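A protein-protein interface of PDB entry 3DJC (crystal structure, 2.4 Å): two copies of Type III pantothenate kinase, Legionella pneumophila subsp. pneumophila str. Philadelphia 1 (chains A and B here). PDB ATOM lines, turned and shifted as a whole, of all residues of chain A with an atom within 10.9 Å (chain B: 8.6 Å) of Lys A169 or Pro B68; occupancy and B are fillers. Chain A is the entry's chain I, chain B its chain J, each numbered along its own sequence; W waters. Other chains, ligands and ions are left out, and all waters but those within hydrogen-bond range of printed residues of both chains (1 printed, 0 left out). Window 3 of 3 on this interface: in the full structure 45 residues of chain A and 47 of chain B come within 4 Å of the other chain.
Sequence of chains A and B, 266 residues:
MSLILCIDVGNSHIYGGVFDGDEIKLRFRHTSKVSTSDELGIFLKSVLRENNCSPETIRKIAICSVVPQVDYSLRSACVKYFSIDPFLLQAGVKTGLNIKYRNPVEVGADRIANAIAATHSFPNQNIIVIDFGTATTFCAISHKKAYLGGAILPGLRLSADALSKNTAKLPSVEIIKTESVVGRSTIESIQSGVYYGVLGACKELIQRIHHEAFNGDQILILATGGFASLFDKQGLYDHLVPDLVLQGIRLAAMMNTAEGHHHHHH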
ATOM      1  N   ALA A 160     -22.481  10.998  -1.270  1.00  0.00           N
ATOM      2  CA  ALA A 160     -21.658  10.670  -2.430  1.00  0.00           C
ATOM      3  C   ALA A 160     -21.206  11.918  -3.200  1.00  0.00           C
ATOM      4  O   ALA A 160     -20.036  12.032  -3.573  1.00  0.00           O
ATOM      5  CB  ALA A 160     -22.403   9.720  -3.347  1.00  0.00           C
ATOM      6  N   ALA A 162     -21.014  15.003  -2.060  1.00  0.00           N
ATOM      7  CA  ALA A 162     -20.164  15.849  -1.212  1.00  0.00           C
ATOM      8  C   ALA A 162     -18.699  15.463  -1.333  1.00  0.00           C
ATOM      9  O   ALA A 162     -17.822  16.323  -1.337  1.00  0.00           O
ATOM     10  CB  ALA A 162     -20.604  15.787   0.244  1.00  0.00           C
ATOM     11  N   LEU A 163     -18.444  14.164  -1.446  1.00  0.00           N
ATOM     12  CA  LEU A 163     -17.087  13.658  -1.602  1.00  0.00           C
ATOM     13  C   LEU A 163     -16.405  14.039  -2.919  1.00  0.00           C
ATOM     14  O   LEU A 163     -15.186  14.114  -2.965  1.00  0.00           O
ATOM     15  CB  LEU A 163     -17.050  12.138  -1.400  1.00  0.00           C
ATOM     16  CG  LEU A 163     -16.728  11.683   0.025  1.00  0.00           C
ATOM     17  CD1 LEU A 163     -17.048  10.220   0.226  1.00  0.00           C
ATOM     18  CD2 LEU A 163     -15.269  11.953   0.344  1.00  0.00           C
ATOM     19  N   SER A 164     -17.185  14.284  -3.971  1.00  0.00           N
ATOM     20  CA  SER A 164     -16.632  14.574  -5.297  1.00  0.00           C
ATOM     21  C   SER A 164     -16.603  16.061  -5.647  1.00  0.00           C
ATOM     22  O   SER A 164     -15.638  16.539  -6.246  1.00  0.00           O
ATOM     23  CB  SER A 164     -17.389  13.799  -6.376  1.00  0.00           C
ATOM     24  OG  SER A 164     -18.665  14.355  -6.616  1.00  0.00           O
ATOM     25  N   LYS A 165     -17.664  16.777  -5.275  1.00  0.00           N
ATOM     26  CA  LYS A 165     -17.815  18.199  -5.594  1.00  0.00           C
ATOM     27  C   LYS A 165     -16.934  19.082  -4.701  1.00  0.00           C
ATOM     28  O   LYS A 165     -16.499  20.160  -5.116  1.00  0.00           O
ATOM     29  CB  LYS A 165     -19.290  18.604  -5.481  1.00  0.00           C
ATOM     30  CG  LYS A 165     -19.681  19.914  -6.170  1.00  0.00           C
ATOM     31  CD  LYS A 165     -21.171  20.210  -5.994  1.00  0.00           C
ATOM     32  CE  LYS A 165     -21.530  20.515  -4.536  1.00  0.00           C
ATOM     33  NZ  LYS A 165     -22.994  20.399  -4.270  1.00  0.00           N
ATOM     34  N   ASN A 166     -16.669  18.614  -3.481  1.00  0.00           N
ATOM     35  CA  ASN A 166     -15.827  19.343  -2.529  1.00  0.00           C
ATOM     36  C   ASN A 166     -14.392  18.804  -2.471  1.00  0.00           C
ATOM     37  O   ASN A 166     -13.671  19.025  -1.491  1.00  0.00           O
ATOM     38  CB  ASN A 166     -16.454  19.326  -1.128  1.00  0.00           C
ATOM     39  CG  ASN A 166     -17.926  19.720  -1.128  1.00  0.00           C
ATOM     40  OD1 ASN A 166     -18.434  20.316  -2.079  1.00  0.00           O
ATOM     41  ND2 ASN A 166     -18.618  19.388  -0.044  1.00  0.00           N
ATOM     42  N   THR A 167     -13.989  18.102  -3.531  1.00  0.00           N
ATOM     43  CA  THR A 167     -12.662  17.493  -3.636  1.00  0.00           C
ATOM     44  C   THR A 167     -12.122  17.671  -5.059  1.00  0.00           C
ATOM     45  O   THR A 167     -12.878  17.625  -6.027  1.00  0.00           O
ATOM     46  CB  THR A 167     -12.710  15.976  -3.267  1.00  0.00           C
ATOM     47  OG1 THR A 167     -13.347  15.802  -1.996  1.00  0.00           O
ATOM     48  CG2 THR A 167     -11.330  15.351  -3.187  1.00  0.00           C
ATOM     49  N   ALA A 168     -10.819  17.915  -5.169  1.00  0.00           N
ATOM     50  CA  ALA A 168     -10.106  17.772  -6.430  1.00  0.00           C
ATOM     51  C   ALA A 168      -9.555  16.352  -6.472  1.00  0.00           C
ATOM     52  O   ALA A 168      -8.978  15.883  -5.486  1.00  0.00           O
ATOM     53  CB  ALA A 168      -8.983  18.788  -6.534  1.00  0.00           C
ATOM     54  N   LYS A 169      -9.752  15.683  -7.610  1.00  0.00           N
ATOM     55  CA  LYS A 169      -9.348  14.280  -7.840  1.00  0.00           C
ATOM     56  C   LYS A 169     -10.093  13.260  -6.960  1.00  0.00           C
ATOM     57  O   LYS A 169      -9.500  12.614  -6.089  1.00  0.00           O
ATOM     58  CB  LYS A 169      -7.817  14.088  -7.761  1.00  0.00           C
ATOM     59  CG  LYS A 169      -7.001  14.871  -8.792  1.00  0.00           C
ATOM     60  CD  LYS A 169      -7.000  14.195 -10.160  1.00  0.00           C
ATOM     61  CE  LYS A 169      -5.813  14.642 -11.006  1.00  0.00           C
ATOM     62  NZ  LYS A 169      -4.519  14.087 -10.505  1.00  0.00           N
ATOM     63  N   LEU A 170     -11.399  13.142  -7.208  1.00  0.00           N
ATOM     64  CA  LEU A 170     -12.273  12.136  -6.596  1.00  0.00           C
ATOM     65  C   LEU A 170     -13.581  12.139  -7.386  1.00  0.00           C
ATOM     66  O   LEU A 170     -14.261  13.167  -7.440  1.00  0.00           O
ATOM     67  CB  LEU A 170     -12.547  12.455  -5.120  1.00  0.00           C
ATOM     68  CG  LEU A 170     -12.845  11.321  -4.132  1.00  0.00           C
ATOM     69  CD1 LEU A 170     -12.278  11.644  -2.748  1.00  0.00           C
ATOM     70  CD2 LEU A 170     -14.340  11.005  -4.045  1.00  0.00           C
ATOM     71  N   PRO A 171     -13.932  10.996  -8.016  1.00  0.00           N
ATOM     72  CA  PRO A 171     -15.134  10.915  -8.859  1.00  0.00           C
ATOM     73  C   PRO A 171     -16.434  10.760  -8.068  1.00  0.00           C
ATOM     74  O   PRO A 171     -16.404  10.340  -6.906  1.00  0.00           O
ATOM     75  CB  PRO A 171     -14.882   9.660  -9.698  1.00  0.00           C
ATOM     76  CG  PRO A 171     -14.033   8.791  -8.824  1.00  0.00           C
ATOM     77  CD  PRO A 171     -13.199   9.714  -7.972  1.00  0.00           C
ATOM     78  N   SER A 172     -17.560  11.115  -8.692  1.00  0.00           N
ATOM     79  CA  SER A 172     -18.885  10.805  -8.136  1.00  0.00           C
ATOM     80  C   SER A 172     -19.286   9.370  -8.500  1.00  0.00           C
ATOM     81  O   SER A 172     -19.109   8.933  -9.641  1.00  0.00           O
ATOM     82  CB  SER A 172     -19.955  11.845  -8.533  1.00  0.00           C
ATOM     83  OG  SER A 172     -19.809  12.316  -9.862  1.00  0.00           O
ATOM     84  N   VAL A 173     -19.815   8.648  -7.515  1.00  0.00           N
ATOM     85  CA  VAL A 173     -19.932   7.191  -7.591  1.00  0.00           C
ATOM     86  C   VAL A 173     -21.395   6.710  -7.629  1.00  0.00           C
ATOM     87  O   VAL A 173     -22.306   7.454  -7.253  1.00  0.00           O
ATOM     88  CB  VAL A 173     -19.116   6.529  -6.426  1.00  0.00           C
ATOM     89  CG1 VAL A 173     -19.978   6.267  -5.191  1.00  0.00           C
ATOM     90  CG2 VAL A 173     -18.440   5.263  -6.885  1.00  0.00           C
ATOM     91  N   SER A 185     -10.190   0.125  -4.869  1.00  0.00           N
ATOM     92  CA  SER A 185     -10.208   1.189  -5.863  1.00  0.00           C
ATOM     93  C   SER A 185     -10.911   2.373  -5.214  1.00  0.00           C
ATOM     94  O   SER A 185     -11.541   2.221  -4.167  1.00  0.00           O
ATOM     95  CB  SER A 185     -10.916   0.750  -7.150  1.00  0.00           C
ATOM     96  OG  SER A 185     -12.316   0.944  -7.075  1.00  0.00           O
ATOM     97  N   THR A 186     -10.770   3.557  -5.809  1.00  0.00           N
ATOM     98  CA  THR A 186     -11.380   4.778  -5.258  1.00  0.00           C
ATOM     99  C   THR A 186     -12.900   4.662  -5.294  1.00  0.00           C
ATOM    100  O   THR A 186     -13.557   4.891  -4.287  1.00  0.00           O
ATOM    101  CB  THR A 186     -10.878   6.051  -5.979  1.00  0.00           C
ATOM    102  OG1 THR A 186      -9.474   6.197  -5.735  1.00  0.00           O
ATOM    103  CG2 THR A 186     -11.598   7.307  -5.478  1.00  0.00           C
ATOM    104  N   ILE A 187     -13.422   4.261  -6.451  1.00  0.00           N
ATOM    105  CA  ILE A 187     -14.833   3.918  -6.655  1.00  0.00           C
ATOM    106  C   ILE A 187     -15.354   2.907  -5.617  1.00  0.00           C
ATOM    107  O   ILE A 187     -16.430   3.097  -5.047  1.00  0.00           O
ATOM    108  CB  ILE A 187     -15.049   3.421  -8.123  1.00  0.00           C
ATOM    109  CG1 ILE A 187     -15.096   4.620  -9.082  1.00  0.00           C
ATOM    110  CG2 ILE A 187     -16.295   2.540  -8.267  1.00  0.00           C
ATOM    111  CD1 ILE A 187     -14.465   4.358 -10.437  1.00  0.00           C
ATOM    112  N   SER A 189     -13.869   2.176  -2.629  1.00  0.00           N
ATOM    113  CA  SER A 189     -13.666   2.733  -1.285  1.00  0.00           C
ATOM    114  C   SER A 189     -14.805   3.644  -0.829  1.00  0.00           C
ATOM    115  O   SER A 189     -15.243   3.562   0.322  1.00  0.00           O
ATOM    116  CB  SER A 189     -12.334   3.492  -1.200  1.00  0.00           C
ATOM    117  OG  SER A 189     -11.226   2.612  -1.264  1.00  0.00           O
ATOM    118  N   ILE A 190     -15.273   4.511  -1.726  1.00  0.00           N
ATOM    119  CA  ILE A 190     -16.410   5.386  -1.419  1.00  0.00           C
ATOM    120  C   ILE A 190     -17.698   4.564  -1.277  1.00  0.00           C
ATOM    121  O   ILE A 190     -18.434   4.766  -0.323  1.00  0.00           O
ATOM    122  CB  ILE A 190     -16.525   6.634  -2.383  1.00  0.00           C
ATOM    123  CG1 ILE A 190     -17.855   7.382  -2.193  1.00  0.00           C
ATOM    124  CG2 ILE A 190     -16.332   6.242  -3.834  1.00  0.00           C
ATOM    125  CD1 ILE A 190     -18.002   8.642  -3.034  1.00  0.00           C
ATOM    126  N   VAL B   9      -0.795  18.911   1.887  1.00  0.00           N
ATOM    127  CA  VAL B   9      -1.797  19.650   1.127  1.00  0.00           C
ATOM    128  C   VAL B   9      -3.099  18.864   1.151  1.00  0.00           C
ATOM    129  O   VAL B   9      -3.162  17.727   0.668  1.00  0.00           O
ATOM    130  CB  VAL B   9      -1.364  19.905  -0.341  1.00  0.00           C
ATOM    131  CG1 VAL B   9      -2.412  20.724  -1.070  1.00  0.00           C
ATOM    132  CG2 VAL B   9      -0.024  20.617  -0.395  1.00  0.00           C
ATOM    133  N   GLY B  10      -4.131  19.469   1.732  1.00  0.00           N
ATOM    134  CA  GLY B  10      -5.443  18.839   1.819  1.00  0.00           C
ATOM    135  C   GLY B  10      -6.439  19.453   0.860  1.00  0.00           C
ATOM    136  O   GLY B  10      -6.077  20.262   0.008  1.00  0.00           O
ATOM    137  N   ASN B  11      -7.698  19.062   1.010  1.00  0.00           N
ATOM    138  CA  ASN B  11      -8.778  19.593   0.194  1.00  0.00           C
ATOM    139  C   ASN B  11      -9.382  20.872   0.780  1.00  0.00           C
ATOM    140  O   ASN B  11     -10.097  21.600   0.089  1.00  0.00           O
ATOM    141  CB  ASN B  11      -9.846  18.520  -0.035  1.00  0.00           C
ATOM    142  CG  ASN B  11      -9.356  17.395  -0.935  1.00  0.00           C
ATOM    143  OD1 ASN B  11      -9.148  16.266  -0.486  1.00  0.00           O
ATOM    144  ND2 ASN B  11      -9.156  17.705  -2.213  1.00  0.00           N
ATOM    145  N   SER B  65       0.854  15.691  -1.182  1.00  0.00           N
ATOM    146  CA  SER B  65      -0.237  16.472  -1.769  1.00  0.00           C
ATOM    147  C   SER B  65      -1.355  15.645  -2.400  1.00  0.00           C
ATOM    148  O   SER B  65      -1.095  14.700  -3.152  1.00  0.00           O
ATOM    149  CB  SER B  65       0.321  17.445  -2.811  1.00  0.00           C
ATOM    150  OG  SER B  65      -0.718  18.094  -3.530  1.00  0.00           O
ATOM    151  N   VAL B  66      -2.595  16.035  -2.103  1.00  0.00           N
ATOM    152  CA  VAL B  66      -3.787  15.408  -2.677  1.00  0.00           C
ATOM    153  C   VAL B  66      -4.494  16.351  -3.667  1.00  0.00           C
ATOM    154  O   VAL B  66      -5.372  15.927  -4.428  1.00  0.00           O
ATOM    155  CB  VAL B  66      -4.748  14.879  -1.567  1.00  0.00           C
ATOM    156  CG1 VAL B  66      -5.626  15.992  -0.990  1.00  0.00           C
ATOM    157  CG2 VAL B  66      -5.586  13.709  -2.072  1.00  0.00           C
ATOM    158  N   VAL B  67      -4.102  17.626  -3.654  1.00  0.00           N
ATOM    159  CA  VAL B  67      -4.577  18.595  -4.643  1.00  0.00           C
ATOM    160  C   VAL B  67      -3.422  18.975  -5.578  1.00  0.00           C
ATOM    161  O   VAL B  67      -2.528  19.732  -5.193  1.00  0.00           O
ATOM    162  CB  VAL B  67      -5.222  19.851  -3.991  1.00  0.00           C
ATOM    163  CG1 VAL B  67      -5.684  20.842  -5.053  1.00  0.00           C
ATOM    164  CG2 VAL B  67      -6.405  19.453  -3.144  1.00  0.00           C
ATOM    165  N   PRO B  68      -3.432  18.429  -6.811  1.00  0.00           N
ATOM    166  CA  PRO B  68      -2.382  18.645  -7.813  1.00  0.00           C
ATOM    167  C   PRO B  68      -2.359  20.045  -8.450  1.00  0.00           C
ATOM    168  O   PRO B  68      -1.472  20.338  -9.255  1.00  0.00           O
ATOM    169  CB  PRO B  68      -2.686  17.576  -8.881  1.00  0.00           C
ATOM    170  CG  PRO B  68      -3.701  16.666  -8.272  1.00  0.00           C
ATOM    171  CD  PRO B  68      -4.467  17.513  -7.319  1.00  0.00           C
ATOM    172  N   GLN B  69      -3.323  20.891  -8.106  1.00  0.00           N
ATOM    173  CA  GLN B  69      -3.353  22.262  -8.610  1.00  0.00           C
ATOM    174  C   GLN B  69      -2.516  23.187  -7.723  1.00  0.00           C
ATOM    175  O   GLN B  69      -2.063  24.244  -8.164  1.00  0.00           O
ATOM    176  CB  GLN B  69      -4.798  22.759  -8.725  1.00  0.00           C
ATOM    177  CG  GLN B  69      -5.614  22.019  -9.784  1.00  0.00           C
ATOM    178  CD  GLN B  69      -7.106  22.061  -9.520  1.00  0.00           C
ATOM    179  OE1 GLN B  69      -7.679  23.122  -9.273  1.00  0.00           O
ATOM    180  NE2 GLN B  69      -7.747  20.900  -9.582  1.00  0.00           N
ATOM    181  N   VAL B  70      -2.315  22.766  -6.475  1.00  0.00           N
ATOM    182  CA  VAL B  70      -1.442  23.445  -5.512  1.00  0.00           C
ATOM    183  C   VAL B  70       0.031  23.100  -5.808  1.00  0.00           C
ATOM    184  O   VAL B  70       0.935  23.869  -5.471  1.00  0.00           O
ATOM    185  CB  VAL B  70      -1.827  23.052  -4.040  1.00  0.00           C
ATOM    186  CG1 VAL B  70      -0.910  23.688  -3.009  1.00  0.00           C
ATOM    187  CG2 VAL B  70      -3.270  23.432  -3.731  1.00  0.00           C
ATOM    188  N   ASP B  71       0.240  21.962  -6.479  1.00  0.00           N
ATOM    189  CA  ASP B  71       1.563  21.355  -6.726  1.00  0.00           C
ATOM    190  C   ASP B  71       2.652  22.239  -7.330  1.00  0.00           C
ATOM    191  O   ASP B  71       3.722  22.381  -6.736  1.00  0.00           O
ATOM    192  CB  ASP B  71       1.418  20.095  -7.589  1.00  0.00           C
ATOM    193  CG  ASP B  71       1.078  18.865  -6.779  1.00  0.00           C
ATOM    194  OD1 ASP B  71       0.970  18.978  -5.540  1.00  0.00           O
ATOM    195  OD2 ASP B  71       0.916  17.784  -7.385  1.00  0.00           O
ATOM    196  N   TYR B  72       2.387  22.811  -8.505  1.00  0.00           N
ATOM    197  CA  TYR B  72       3.411  23.562  -9.243  1.00  0.00           C
ATOM    198  C   TYR B  72       3.885  24.832  -8.531  1.00  0.00           C
ATOM    199  O   TYR B  72       5.090  25.077  -8.434  1.00  0.00           O
ATOM    200  CB  TYR B  72       2.962  23.892 -10.676  1.00  0.00           C
ATOM    201  CG  TYR B  72       4.006  24.672 -11.448  1.00  0.00           C
ATOM    202  CD1 TYR B  72       5.215  24.078 -11.817  1.00  0.00           C
ATOM    203  CD2 TYR B  72       3.800  26.012 -11.788  1.00  0.00           C
ATOM    204  CE1 TYR B  72       6.189  24.790 -12.511  1.00  0.00           C
ATOM    205  CE2 TYR B  72       4.769  26.734 -12.486  1.00  0.00           C
ATOM    206  CZ  TYR B  72       5.961  26.115 -12.844  1.00  0.00           C
ATOM    207  OH  TYR B  72       6.925  26.815 -13.534  1.00  0.00           O
ATOM    208  N   SER B  73       2.936  25.628  -8.040  1.00  0.00           N
ATOM    209  CA  SER B  73       3.244  26.896  -7.379  1.00  0.00           C
ATOM    210  C   SER B  73       3.904  26.716  -6.008  1.00  0.00           C
ATOM    211  O   SER B  73       4.670  27.571  -5.577  1.00  0.00           O
ATOM    212  CB  SER B  73       1.990  27.767  -7.277  1.00  0.00           C
ATOM    213  OG  SER B  73       0.836  26.971  -7.077  1.00  0.00           O
ATOM    214  N   LEU B  74       3.609  25.606  -5.334  1.00  0.00           N
ATOM    215  CA  LEU B  74       4.246  25.278  -4.058  1.00  0.00           C
ATOM    216  C   LEU B  74       5.669  24.777  -4.279  1.00  0.00           C
ATOM    217  O   LEU B  74       6.538  25.001  -3.437  1.00  0.00           O
ATOM    218  CB  LEU B  74       3.421  24.246  -3.278  1.00  0.00           C
ATOM    219  CG  LEU B  74       3.793  23.875  -1.834  1.00  0.00           C
ATOM    220  CD1 LEU B  74       3.661  25.040  -0.865  1.00  0.00           C
ATOM    221  CD2 LEU B  74       2.951  22.712  -1.367  1.00  0.00           C
ATOM    222  N   VAL B 105      -1.284   3.624  -7.539  1.00  0.00           N
ATOM    223  CA  VAL B 105      -1.183   5.065  -7.802  1.00  0.00           C
ATOM    224  C   VAL B 105      -2.420   5.839  -7.313  1.00  0.00           C
ATOM    225  O   VAL B 105      -2.298   6.981  -6.852  1.00  0.00           O
ATOM    226  CB  VAL B 105      -0.957   5.356  -9.315  1.00  0.00           C
ATOM    227  CG1 VAL B 105      -0.354   6.737  -9.514  1.00  0.00           C
ATOM    228  CG2 VAL B 105      -0.055   4.304  -9.950  1.00  0.00           C
ATOM    229  N   GLU B 106      -3.589   5.196  -7.386  1.00  0.00           N
ATOM    230  CA  GLU B 106      -4.813   5.912  -7.023  1.00  0.00           C
ATOM    231  C   GLU B 106      -5.056   6.036  -5.510  1.00  0.00           C
ATOM    232  O   GLU B 106      -5.991   6.733  -5.090  1.00  0.00           O
ATOM    233  CB  GLU B 106      -6.044   5.446  -7.822  1.00  0.00           C
ATOM    234  CG  GLU B 106      -6.738   4.172  -7.372  1.00  0.00           C
ATOM    235  CD  GLU B 106      -8.038   3.939  -8.136  1.00  0.00           C
ATOM    236  OE1 GLU B 106      -8.323   2.781  -8.503  1.00  0.00           O
ATOM    237  OE2 GLU B 106      -8.771   4.919  -8.387  1.00  0.00           O
ATOM    238  N   GLY B 108      -4.229   7.972  -2.391  1.00  0.00           N
ATOM    239  CA  GLY B 108      -3.783   9.341  -2.151  1.00  0.00           C
ATOM    240  C   GLY B 108      -2.482   9.391  -1.375  1.00  0.00           C
ATOM    241  O   GLY B 108      -2.233   8.537  -0.517  1.00  0.00           O
ATOM    242  N   ASP B 110      -1.644  11.180   0.902  1.00  0.00           N
ATOM    243  CA  ASP B 110      -1.959  11.426   2.306  1.00  0.00           C
ATOM    244  C   ASP B 110      -2.291  10.144   3.067  1.00  0.00           C
ATOM    245  O   ASP B 110      -2.114  10.078   4.290  1.00  0.00           O
ATOM    246  CB  ASP B 110      -3.099  12.454   2.431  1.00  0.00           C
ATOM    247  CG  ASP B 110      -4.339  12.057   1.662  1.00  0.00           C
ATOM    248  OD1 ASP B 110      -4.243  11.773   0.448  1.00  0.00           O
ATOM    249  OD2 ASP B 110      -5.424  12.046   2.276  1.00  0.00           O
ATOM    250  N   ILE B 152     -14.051   5.146   2.381  1.00  0.00           N
ATOM    251  CA  ILE B 152     -14.053   6.612   2.384  1.00  0.00           C
ATOM    252  C   ILE B 152     -15.474   7.155   2.593  1.00  0.00           C
ATOM    253  O   ILE B 152     -16.355   6.953   1.757  1.00  0.00           O
ATOM    254  CB  ILE B 152     -13.461   7.225   1.077  1.00  0.00           C
ATOM    255  CG1 ILE B 152     -12.023   6.758   0.818  1.00  0.00           C
ATOM    256  CG2 ILE B 152     -13.493   8.747   1.136  1.00  0.00           C
ATOM    257  CD1 ILE B 152     -11.490   7.131  -0.574  1.00  0.00           C
HETATM  258  O   HOH W   1      -8.685   8.074  -8.416  1.00  0.00           O
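Of the printed residues of chain B, Leu A163 touches Ile B152 (3.7 Å).
Printed residues of chain B within 4 Å of Thr A167: Asn B11 (3.3 Å).
Of chain B, only Asn B11 (3.4 Å), Val B66 (3.8 Å) and Gln B69 (3.9 Å) come within 4 Å of Ala A168.
Of chain B, only Pro B68 (3.5 Å) comes within 4 Å of Lys A169.
Leu A170 touches none of the printed residues of chain B.
Printed residues of chain A within 4 Å of Asn B11: Thr A167 (3.3 Å) and Ala A168 (3.4 Å).
Val B67 touches none of the printed residues of chain A.
Of chain A, only Lys A169 comes within 4 Å of Pro B68.
Gln B69 touches just one residue of chain A: Ala A168 (3.9 Å).
No residue of chain A comes within 4 Å of Val B70.
No residue of chain A comes within 4 Å of Asp B71.
Of the printed residues of chain A, Ile B152 touches Leu A163, Ser A189 and Ile A190.
The nearest printed residue of chain B that does not touch Thr A167 is Val B66 (6.1 Å).
Water W1 lies within hydrogen-bond range of the side-chain carboxylate (OE2) of Glu B106 (3.2 Å) and the side-chain hydroxyl (OG1) of Thr A186 (3.4 Å).
O of Ile B152 touches CD1 of Leu A163 (3.7 Å).
Thr A167 touches Asn B11.
Val B66 touches Ala A168.
Ala A168 touches Gln B69.
Pro B68 touches Lys A169.
Ser A185 touches Glu B106 (CB to OE1, 3.6 Å).
Ile B152 touches Ile A190.
The side-chain hydroxyl of Thr A167 sits at hydrogen-bond distance from the backbone carbonyl oxygen of Leu A163, at 2.7 Å.
O of Ser A185 is in hydrogen-bond range of OG of Ser A189 (2.9 Å).
The backbone NH of Val B66 sits at hydrogen-bond distance from the backbone carbonyl oxygen of Val B9 (3.3 Å).
Of the 18 printed residues of chain A, 8 touch a printed residue of chain B.
Hydrophobic or aromatic side chains of chain A that line the printed part of chain B: Leu A163 and Ala A168.
Among the printed residues, no Asp or Glu carboxylate lies within 4 Å of a Lys or Arg side-chain nitrogen of the other chain.
ND2 of Asn B11 sits close to N of Ala A168 (3.4 Å).
The side-chain carboxylate of Glu B106 sits at hydrogen-bond distance from the side-chain hydroxyl of Thr A186, 3.0 Å away.
The backbone carbonyl oxygen (O) of Ser A189 is in hydrogen-bond range of the backbone NH (N) of Ile B152, at 2.9 Å.
No position is printed for both chains.
Of the 10 pairs that touch across the chains among the printed residues, none has its exchanged pair printed and touching as well.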
